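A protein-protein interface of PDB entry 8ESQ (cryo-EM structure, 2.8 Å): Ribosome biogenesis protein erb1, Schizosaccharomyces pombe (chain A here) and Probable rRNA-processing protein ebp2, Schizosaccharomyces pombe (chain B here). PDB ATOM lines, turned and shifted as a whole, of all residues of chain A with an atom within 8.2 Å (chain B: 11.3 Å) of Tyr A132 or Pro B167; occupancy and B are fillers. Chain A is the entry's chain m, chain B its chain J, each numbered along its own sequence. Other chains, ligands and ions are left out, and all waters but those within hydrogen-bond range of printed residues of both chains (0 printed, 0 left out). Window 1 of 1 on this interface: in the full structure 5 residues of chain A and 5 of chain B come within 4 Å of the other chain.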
ATOM      1  N   TYR A 129      15.644 -12.539  14.588  1.00  0.00           N
ATOM      2  CA  TYR A 129      14.821 -13.622  15.138  1.00  0.00           C
ATOM      3  C   TYR A 129      13.623 -13.922  14.243  1.00  0.00           C
ATOM      4  O   TYR A 129      12.459 -13.885  14.648  1.00  0.00           O
ATOM      5  CB  TYR A 129      14.385 -13.292  16.565  1.00  0.00           C
ATOM      6  CG  TYR A 129      15.516 -13.201  17.580  1.00  0.00           C
ATOM      7  CD1 TYR A 129      16.844 -13.167  17.177  1.00  0.00           C
ATOM      8  CD2 TYR A 129      15.250 -13.181  18.946  1.00  0.00           C
ATOM      9  CE1 TYR A 129      17.874 -13.096  18.093  1.00  0.00           C
ATOM     10  CE2 TYR A 129      16.278 -13.112  19.875  1.00  0.00           C
ATOM     11  CZ  TYR A 129      17.588 -13.069  19.440  1.00  0.00           C
ATOM     12  OH  TYR A 129      18.619 -13.001  20.349  1.00  0.00           O
ATOM     13  N   ILE A 130      13.946 -14.215  12.987  1.00  0.00           N
ATOM     14  CA  ILE A 130      12.946 -14.629  11.986  1.00  0.00           C
ATOM     15  C   ILE A 130      13.035 -16.144  11.847  1.00  0.00           C
ATOM     16  O   ILE A 130      13.543 -16.697  10.873  1.00  0.00           O
ATOM     17  CB  ILE A 130      13.114 -13.871  10.662  1.00  0.00           C
ATOM     18  CG1 ILE A 130      14.595 -13.707  10.219  1.00  0.00           C
ATOM     19  CG2 ILE A 130      12.404 -12.555  10.734  1.00  0.00           C
ATOM     20  CD1 ILE A 130      15.507 -14.913  10.040  1.00  0.00           C
ATOM     21  N   ASN A 131      12.438 -16.841  12.801  1.00  0.00           N
ATOM     22  CA  ASN A 131      12.510 -18.290  12.731  1.00  0.00           C
ATOM     23  C   ASN A 131      11.203 -18.894  12.234  1.00  0.00           C
ATOM     24  O   ASN A 131      11.184 -19.549  11.187  1.00  0.00           O
ATOM     25  CB  ASN A 131      12.907 -18.857  14.094  1.00  0.00           C
ATOM     26  CG  ASN A 131      14.066 -19.818  13.995  1.00  0.00           C
ATOM     27  OD1 ASN A 131      14.090 -20.691  13.124  1.00  0.00           O
ATOM     28  ND2 ASN A 131      15.050 -19.650  14.868  1.00  0.00           N
ATOM     29  N   TYR A 132      10.103 -18.633  12.930  1.00  0.00           N
ATOM     30  CA  TYR A 132       8.802 -19.120  12.506  1.00  0.00           C
ATOM     31  C   TYR A 132       7.723 -18.191  13.043  1.00  0.00           C
ATOM     32  O   TYR A 132       8.000 -17.212  13.744  1.00  0.00           O
ATOM     33  CB  TYR A 132       8.569 -20.566  12.964  1.00  0.00           C
ATOM     34  CG  TYR A 132       9.272 -21.602  12.114  1.00  0.00           C
ATOM     35  CD1 TYR A 132       8.665 -22.129  10.980  1.00  0.00           C
ATOM     36  CD2 TYR A 132      10.530 -22.078  12.462  1.00  0.00           C
ATOM     37  CE1 TYR A 132       9.303 -23.079  10.204  1.00  0.00           C
ATOM     38  CE2 TYR A 132      11.174 -23.018  11.691  1.00  0.00           C
ATOM     39  CZ  TYR A 132      10.558 -23.518  10.567  1.00  0.00           C
ATOM     40  OH  TYR A 132      11.201 -24.465   9.804  1.00  0.00           O
ATOM     41  N   ASP A 133       6.481 -18.513  12.703  1.00  0.00           N
ATOM     42  CA  ASP A 133       5.307 -17.769  13.121  1.00  0.00           C
ATOM     43  C   ASP A 133       4.390 -18.722  13.876  1.00  0.00           C
ATOM     44  O   ASP A 133       4.706 -19.901  14.064  1.00  0.00           O
ATOM     45  CB  ASP A 133       4.598 -17.149  11.907  1.00  0.00           C
ATOM     46  CG  ASP A 133       3.579 -16.098  12.294  1.00  0.00           C
ATOM     47  OD1 ASP A 133       3.345 -15.911  13.506  1.00  0.00           O
ATOM     48  OD2 ASP A 133       3.004 -15.463  11.386  1.00  0.00           O
ATOM     49  N   ILE A 134       3.244 -18.205  14.327  1.00  0.00           N
ATOM     50  CA  ILE A 134       2.239 -19.070  14.927  1.00  0.00           C
ATOM     51  C   ILE A 134       1.800 -20.101  13.895  1.00  0.00           C
ATOM     52  O   ILE A 134       1.796 -19.837  12.686  1.00  0.00           O
ATOM     53  CB  ILE A 134       1.054 -18.244  15.457  1.00  0.00           C
ATOM     54  CG1 ILE A 134       0.309 -19.028  16.536  1.00  0.00           C
ATOM     55  CG2 ILE A 134       0.106 -17.857  14.332  1.00  0.00           C
ATOM     56  CD1 ILE A 134       1.122 -19.244  17.793  1.00  0.00           C
ATOM     57  N   ASP A 135       1.475 -21.302  14.373  1.00  0.00           N
ATOM     58  CA  ASP A 135       1.203 -22.500  13.581  1.00  0.00           C
ATOM     59  C   ASP A 135       2.440 -23.010  12.851  1.00  0.00           C
ATOM     60  O   ASP A 135       2.346 -24.007  12.126  1.00  0.00           O
ATOM     61  CB  ASP A 135       0.070 -22.300  12.564  1.00  0.00           C
ATOM     62  CG  ASP A 135      -1.251 -21.961  13.224  1.00  0.00           C
ATOM     63  OD1 ASP A 135      -1.446 -22.347  14.396  1.00  0.00           O
ATOM     64  OD2 ASP A 135      -2.095 -21.313  12.570  1.00  0.00           O
ATOM     65  N   GLY A 136       3.594 -22.367  13.019  1.00  0.00           N
ATOM     66  CA  GLY A 136       4.849 -22.881  12.505  1.00  0.00           C
ATOM     67  C   GLY A 136       5.071 -22.736  11.015  1.00  0.00           C
ATOM     68  O   GLY A 136       5.126 -23.734  10.293  1.00  0.00           O
ATOM     69  N   LYS A 137       5.197 -21.501  10.533  1.00  0.00           N
ATOM     70  CA  LYS A 137       5.542 -21.244   9.139  1.00  0.00           C
ATOM     71  C   LYS A 137       6.618 -20.173   9.095  1.00  0.00           C
ATOM     72  O   LYS A 137       6.478 -19.130   9.740  1.00  0.00           O
ATOM     73  CB  LYS A 137       4.316 -20.808   8.328  1.00  0.00           C
ATOM     74  CG  LYS A 137       3.169 -21.803   8.353  1.00  0.00           C
ATOM     75  CD  LYS A 137       1.837 -21.123   8.091  1.00  0.00           C
ATOM     76  CE  LYS A 137       1.601 -19.973   9.053  1.00  0.00           C
ATOM     77  NZ  LYS A 137       1.839 -20.381  10.464  1.00  0.00           N
ATOM     78  N   LYS A 138       7.692 -20.431   8.349  1.00  0.00           N
ATOM     79  CA  LYS A 138       8.741 -19.432   8.203  1.00  0.00           C
ATOM     80  C   LYS A 138       8.200 -18.199   7.496  1.00  0.00           C
ATOM     81  O   LYS A 138       7.609 -18.294   6.417  1.00  0.00           O
ATOM     82  CB  LYS A 138       9.928 -19.998   7.422  1.00  0.00           C
ATOM     83  CG  LYS A 138      10.917 -20.785   8.259  1.00  0.00           C
ATOM     84  CD  LYS A 138      12.235 -20.970   7.522  1.00  0.00           C
ATOM     85  CE  LYS A 138      13.214 -21.807   8.330  1.00  0.00           C
ATOM     86  NZ  LYS A 138      13.607 -21.138   9.600  1.00  0.00           N
ATOM     87  N   ILE A 139       8.406 -17.047   8.105  1.00  0.00           N
ATOM     88  CA  ILE A 139       8.044 -15.777   7.492  1.00  0.00           C
ATOM     89  C   ILE A 139       9.250 -15.248   6.736  1.00  0.00           C
ATOM     90  O   ILE A 139      10.397 -15.400   7.176  1.00  0.00           O
ATOM     91  CB  ILE A 139       7.545 -14.774   8.549  1.00  0.00           C
ATOM     92  CG1 ILE A 139       8.582 -14.593   9.660  1.00  0.00           C
ATOM     93  CG2 ILE A 139       6.213 -15.229   9.119  1.00  0.00           C
ATOM     94  CD1 ILE A 139       8.247 -13.473  10.620  1.00  0.00           C
ATOM     95  N   MET A 168      10.915  -9.469  14.598  1.00  0.00           N
ATOM     96  CA  MET A 168      10.495  -9.855  13.256  1.00  0.00           C
ATOM     97  C   MET A 168      11.327  -9.146  12.193  1.00  0.00           C
ATOM     98  O   MET A 168      12.039  -9.785  11.417  1.00  0.00           O
ATOM     99  CB  MET A 168       9.004  -9.564  13.078  1.00  0.00           C
ATOM    100  CG  MET A 168       8.118 -10.296  14.077  1.00  0.00           C
ATOM    101  SD  MET A 168       8.789 -11.895  14.579  1.00  0.00           S
ATOM    102  CE  MET A 168       7.353 -12.647  15.343  1.00  0.00           C
ATOM    103  N   VAL B 162      -0.477 -30.171  11.400  1.00  0.00           N
ATOM    104  CA  VAL B 162       0.272 -29.333  12.327  1.00  0.00           C
ATOM    105  C   VAL B 162       1.695 -29.860  12.413  1.00  0.00           C
ATOM    106  O   VAL B 162       1.926 -31.063  12.575  1.00  0.00           O
ATOM    107  CB  VAL B 162      -0.398 -29.305  13.717  1.00  0.00           C
ATOM    108  CG1 VAL B 162       0.381 -28.409  14.664  1.00  0.00           C
ATOM    109  CG2 VAL B 162      -1.842 -28.851  13.595  1.00  0.00           C
ATOM    110  N   LEU B 163       2.663 -28.951  12.313  1.00  0.00           N
ATOM    111  CA  LEU B 163       4.072 -29.335  12.318  1.00  0.00           C
ATOM    112  C   LEU B 163       4.428 -29.850  13.704  1.00  0.00           C
ATOM    113  O   LEU B 163       4.604 -29.075  14.646  1.00  0.00           O
ATOM    114  CB  LEU B 163       4.973 -28.174  11.914  1.00  0.00           C
ATOM    115  CG  LEU B 163       4.809 -27.487  10.553  1.00  0.00           C
ATOM    116  CD1 LEU B 163       3.570 -26.598  10.466  1.00  0.00           C
ATOM    117  CD2 LEU B 163       6.073 -26.714  10.206  1.00  0.00           C
ATOM    118  N   ILE B 164       4.522 -31.172  13.831  1.00  0.00           N
ATOM    119  CA  ILE B 164       4.863 -31.770  15.115  1.00  0.00           C
ATOM    120  C   ILE B 164       6.301 -31.443  15.493  1.00  0.00           C
ATOM    121  O   ILE B 164       6.587 -31.033  16.624  1.00  0.00           O
ATOM    122  CB  ILE B 164       4.625 -33.289  15.074  1.00  0.00           C
ATOM    123  CG1 ILE B 164       3.130 -33.610  14.950  1.00  0.00           C
ATOM    124  CG2 ILE B 164       5.243 -33.942  16.285  1.00  0.00           C
ATOM    125  CD1 ILE B 164       2.206 -32.560  15.536  1.00  0.00           C
ATOM    126  N   SER B 165       7.224 -31.611  14.554  1.00  0.00           N
ATOM    127  CA  SER B 165       8.638 -31.467  14.854  1.00  0.00           C
ATOM    128  C   SER B 165       9.017 -30.002  15.014  1.00  0.00           C
ATOM    129  O   SER B 165       8.475 -29.118  14.343  1.00  0.00           O
ATOM    130  CB  SER B 165       9.487 -32.103  13.751  1.00  0.00           C
ATOM    131  OG  SER B 165       9.603 -31.240  12.633  1.00  0.00           O
ATOM    132  N   ARG B 166       9.962 -29.750  15.917  1.00  0.00           N
ATOM    133  CA  ARG B 166      10.545 -28.428  16.047  1.00  0.00           C
ATOM    134  C   ARG B 166      11.760 -28.350  15.142  1.00  0.00           C
ATOM    135  O   ARG B 166      12.727 -29.098  15.355  1.00  0.00           O
ATOM    136  CB  ARG B 166      10.940 -28.138  17.489  1.00  0.00           C
ATOM    137  CG  ARG B 166      11.831 -26.914  17.641  1.00  0.00           C
ATOM    138  CD  ARG B 166      12.268 -26.713  19.081  1.00  0.00           C
ATOM    139  NE  ARG B 166      13.377 -25.771  19.188  1.00  0.00           N
ATOM    140  CZ  ARG B 166      14.657 -26.107  19.108  1.00  0.00           C
ATOM    141  NH1 ARG B 166      15.032 -27.361  18.914  1.00  0.00           N
ATOM    142  NH2 ARG B 166      15.584 -25.160  19.227  1.00  0.00           N
ATOM    143  N   PRO B 167      11.752 -27.491  14.128  1.00  0.00           N
ATOM    144  CA  PRO B 167      12.874 -27.449  13.186  1.00  0.00           C
ATOM    145  C   PRO B 167      14.169 -27.039  13.868  1.00  0.00           C
ATOM    146  O   PRO B 167      14.172 -26.300  14.856  1.00  0.00           O
ATOM    147  CB  PRO B 167      12.427 -26.411  12.150  1.00  0.00           C
ATOM    148  CG  PRO B 167      10.931 -26.388  12.276  1.00  0.00           C
ATOM    149  CD  PRO B 167      10.659 -26.597  13.724  1.00  0.00           C
ATOM    150  N   HIS B 168      15.280 -27.543  13.326  1.00  0.00           N
ATOM    151  CA  HIS B 168      16.591 -27.298  13.914  1.00  0.00           C
ATOM    152  C   HIS B 168      16.939 -25.818  13.967  1.00  0.00           C
ATOM    153  O   HIS B 168      17.782 -25.419  14.776  1.00  0.00           O
ATOM    154  CB  HIS B 168      17.680 -28.041  13.132  1.00  0.00           C
ATOM    155  CG  HIS B 168      17.730 -27.700  11.672  1.00  0.00           C
ATOM    156  ND1 HIS B 168      16.619 -27.329  10.946  1.00  0.00           N
ATOM    157  CD2 HIS B 168      18.771 -27.669  10.805  1.00  0.00           C
ATOM    158  CE1 HIS B 168      16.971 -27.089   9.695  1.00  0.00           C
ATOM    159  NE2 HIS B 168      18.272 -27.288   9.584  1.00  0.00           N
ATOM    160  N   ASP B 169      16.317 -24.998  13.121  1.00  0.00           N
ATOM    161  CA  ASP B 169      16.618 -23.574  13.090  1.00  0.00           C
ATOM    162  C   ASP B 169      15.952 -22.791  14.211  1.00  0.00           C
ATOM    163  O   ASP B 169      16.373 -21.662  14.484  1.00  0.00           O
ATOM    164  CB  ASP B 169      16.202 -22.981  11.744  1.00  0.00           C
ATOM    165  CG  ASP B 169      16.976 -21.728  11.403  1.00  0.00           C
ATOM    166  OD1 ASP B 169      17.864 -21.343  12.193  1.00  0.00           O
ATOM    167  OD2 ASP B 169      16.696 -21.127  10.346  1.00  0.00           O
ATOM    168  N   TYR B 170      14.935 -23.347  14.863  1.00  0.00           N
ATOM    169  CA  TYR B 170      14.195 -22.587  15.860  1.00  0.00           C
ATOM    170  C   TYR B 170      15.060 -22.309  17.083  1.00  0.00           C
ATOM    171  O   TYR B 170      15.699 -23.212  17.630  1.00  0.00           O
ATOM    172  CB  TYR B 170      12.923 -23.324  16.263  1.00  0.00           C
ATOM    173  CG  TYR B 170      11.824 -22.398  16.733  1.00  0.00           C
ATOM    174  CD1 TYR B 170      12.020 -21.020  16.789  1.00  0.00           C
ATOM    175  CD2 TYR B 170      10.592 -22.902  17.125  1.00  0.00           C
ATOM    176  CE1 TYR B 170      11.019 -20.175  17.223  1.00  0.00           C
ATOM    177  CE2 TYR B 170       9.586 -22.067  17.560  1.00  0.00           C
ATOM    178  CZ  TYR B 170       9.803 -20.707  17.608  1.00  0.00           C
ATOM    179  OH  TYR B 170       8.792 -19.884  18.044  1.00  0.00           O
ATOM    180  N   PHE B 171      15.062 -21.049  17.510  1.00  0.00           N
ATOM    181  CA  PHE B 171      15.856 -20.554  18.628  1.00  0.00           C
ATOM    182  C   PHE B 171      14.987 -19.741  19.579  1.00  0.00           C
ATOM    183  O   PHE B 171      15.382 -18.687  20.082  1.00  0.00           O
ATOM    184  CB  PHE B 171      17.031 -19.724  18.121  1.00  0.00           C
ATOM    185  CG  PHE B 171      18.004 -20.500  17.281  1.00  0.00           C
ATOM    186  CD1 PHE B 171      18.482 -21.724  17.713  1.00  0.00           C
ATOM    187  CD2 PHE B 171      18.447 -20.006  16.064  1.00  0.00           C
ATOM    188  CE1 PHE B 171      19.378 -22.445  16.952  1.00  0.00           C
ATOM    189  CE2 PHE B 171      19.345 -20.725  15.295  1.00  0.00           C
ATOM    190  CZ  PHE B 171      19.811 -21.946  15.741  1.00  0.00           C
ATOM    191  N   ALA B 172      13.775 -20.228  19.839  1.00  0.00           N
ATOM    192  CA  ALA B 172      12.914 -19.578  20.812  1.00  0.00           C
ATOM    193  C   ALA B 172      13.406 -19.871  22.227  1.00  0.00           C
ATOM    194  O   ALA B 172      14.216 -20.771  22.464  1.00  0.00           O
ATOM    195  CB  ALA B 172      11.467 -20.036  20.648  1.00  0.00           C
ATOM    196  N   GLU B 173      12.899 -19.094  23.179  1.00  0.00           N
ATOM    197  CA  GLU B 173      13.365 -19.187  24.553  1.00  0.00           C
ATOM    198  C   GLU B 173      12.875 -20.487  25.178  1.00  0.00           C
ATOM    199  O   GLU B 173      11.729 -20.897  24.969  1.00  0.00           O
ATOM    200  CB  GLU B 173      12.885 -17.984  25.361  1.00  0.00           C
ATOM    201  CG  GLU B 173      13.857 -17.564  26.447  1.00  0.00           C
ATOM    202  CD  GLU B 173      13.698 -18.369  27.715  1.00  0.00           C
ATOM    203  OE1 GLU B 173      12.592 -18.891  27.946  1.00  0.00           O
ATOM    204  OE2 GLU B 173      14.680 -18.482  28.479  1.00  0.00           O
ATOM    205  N   MET B 174      13.750 -21.135  25.937  1.00  0.00           N
ATOM    206  CA  MET B 174      13.486 -22.464  26.465  1.00  0.00           C
ATOM    207  C   MET B 174      12.938 -22.359  27.884  1.00  0.00           C
ATOM    208  O   MET B 174      13.239 -21.411  28.612  1.00  0.00           O
ATOM    209  CB  MET B 174      14.773 -23.292  26.466  1.00  0.00           C
ATOM    210  CG  MET B 174      15.024 -24.165  25.228  1.00  0.00           C
ATOM    211  SD  MET B 174      13.614 -24.997  24.468  1.00  0.00           S
ATOM    212  CE  MET B 174      13.085 -23.763  23.285  1.00  0.00           C
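ND2 of Asn A131 sits at hydrogen-bond distance from O of Asp B169 (2.4 Å). The side-chain amino group (NZ) of Lys A138 is in salt-bridge range of the side-chain carboxylate (OD2) of Asp B169, 3.2 Å away. The side-chain amide oxygen of Asn A131 is in hydrogen-bond range of the backbone NH of Tyr B170, at 3.3 Å. N of Phe B171 lies close to ND2 of Asn A131, at 3.0 Å.
NH2 of Arg B166 is in hydrogen-bond range of O of Tyr B170 (2.5 Å). The backbone carbonyl oxygen of Asn A131 lies close to the side-chain amino group of Lys A138, 3.3 Å away.
CG of Pro B167 touches OH of Tyr A132, 3.1 Å away. Asp A135 touches Leu B163. Gly A136 touches Leu B163 (O to CD2, 3.1 Å).
Of chain B, only Pro B167 comes within 4 Å of Tyr A132. Of chain A, only Tyr A132 (3.1 Å) comes within 4 Å of Pro B167. Ile A130 touches none of the printed residues of chain B. Of chain B, only Asp B169 (2.4 Å), Tyr B170 (3.2 Å) and Phe B171 (3.0 Å) come within 4 Å of Asn A131. Of chain B, only Leu B163 (3.1 Å) comes within 4 Å of Gly A136. No residue of chain B comes within 4 Å of Ile A139. Of the printed residues of chain A, Phe B171 touches Asn A131 (3.0 Å). Of the printed residues of chain B, Asp A135 touches Leu B163. Of the printed residues of chain A, Asp B169 touches Asn A131 (2.4 Å) and Lys A138 (3.2 Å). Printed residues of chain A within 4 Å of Tyr B170: Asn A131. Of the printed residues of chain A, Leu B163 touches Asp A135 and Gly A136. His B168 touches none of the printed residues of chain A. Ala B172 touches none of the printed residues of chain A. The nearest residue of chain B that does not touch Tyr A132 is Tyr B170 (4.5 Å). The nearest printed residue of chain B that does not touch Asp A135 is Val B162 (5.4 Å).
Of the 13 printed residues of chain B, 5 touch a printed residue of chain A. Hydrophobic or aromatic side chains of chain B that line the printed part of chain A: Leu B163, Pro B167, Tyr B170 and Phe B171. Of the 12 printed residues of chain A, 5 touch a printed residue of chain B. Hydrophobic or aromatic side chains of chain A that line the printed part of chain B: Tyr A132.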
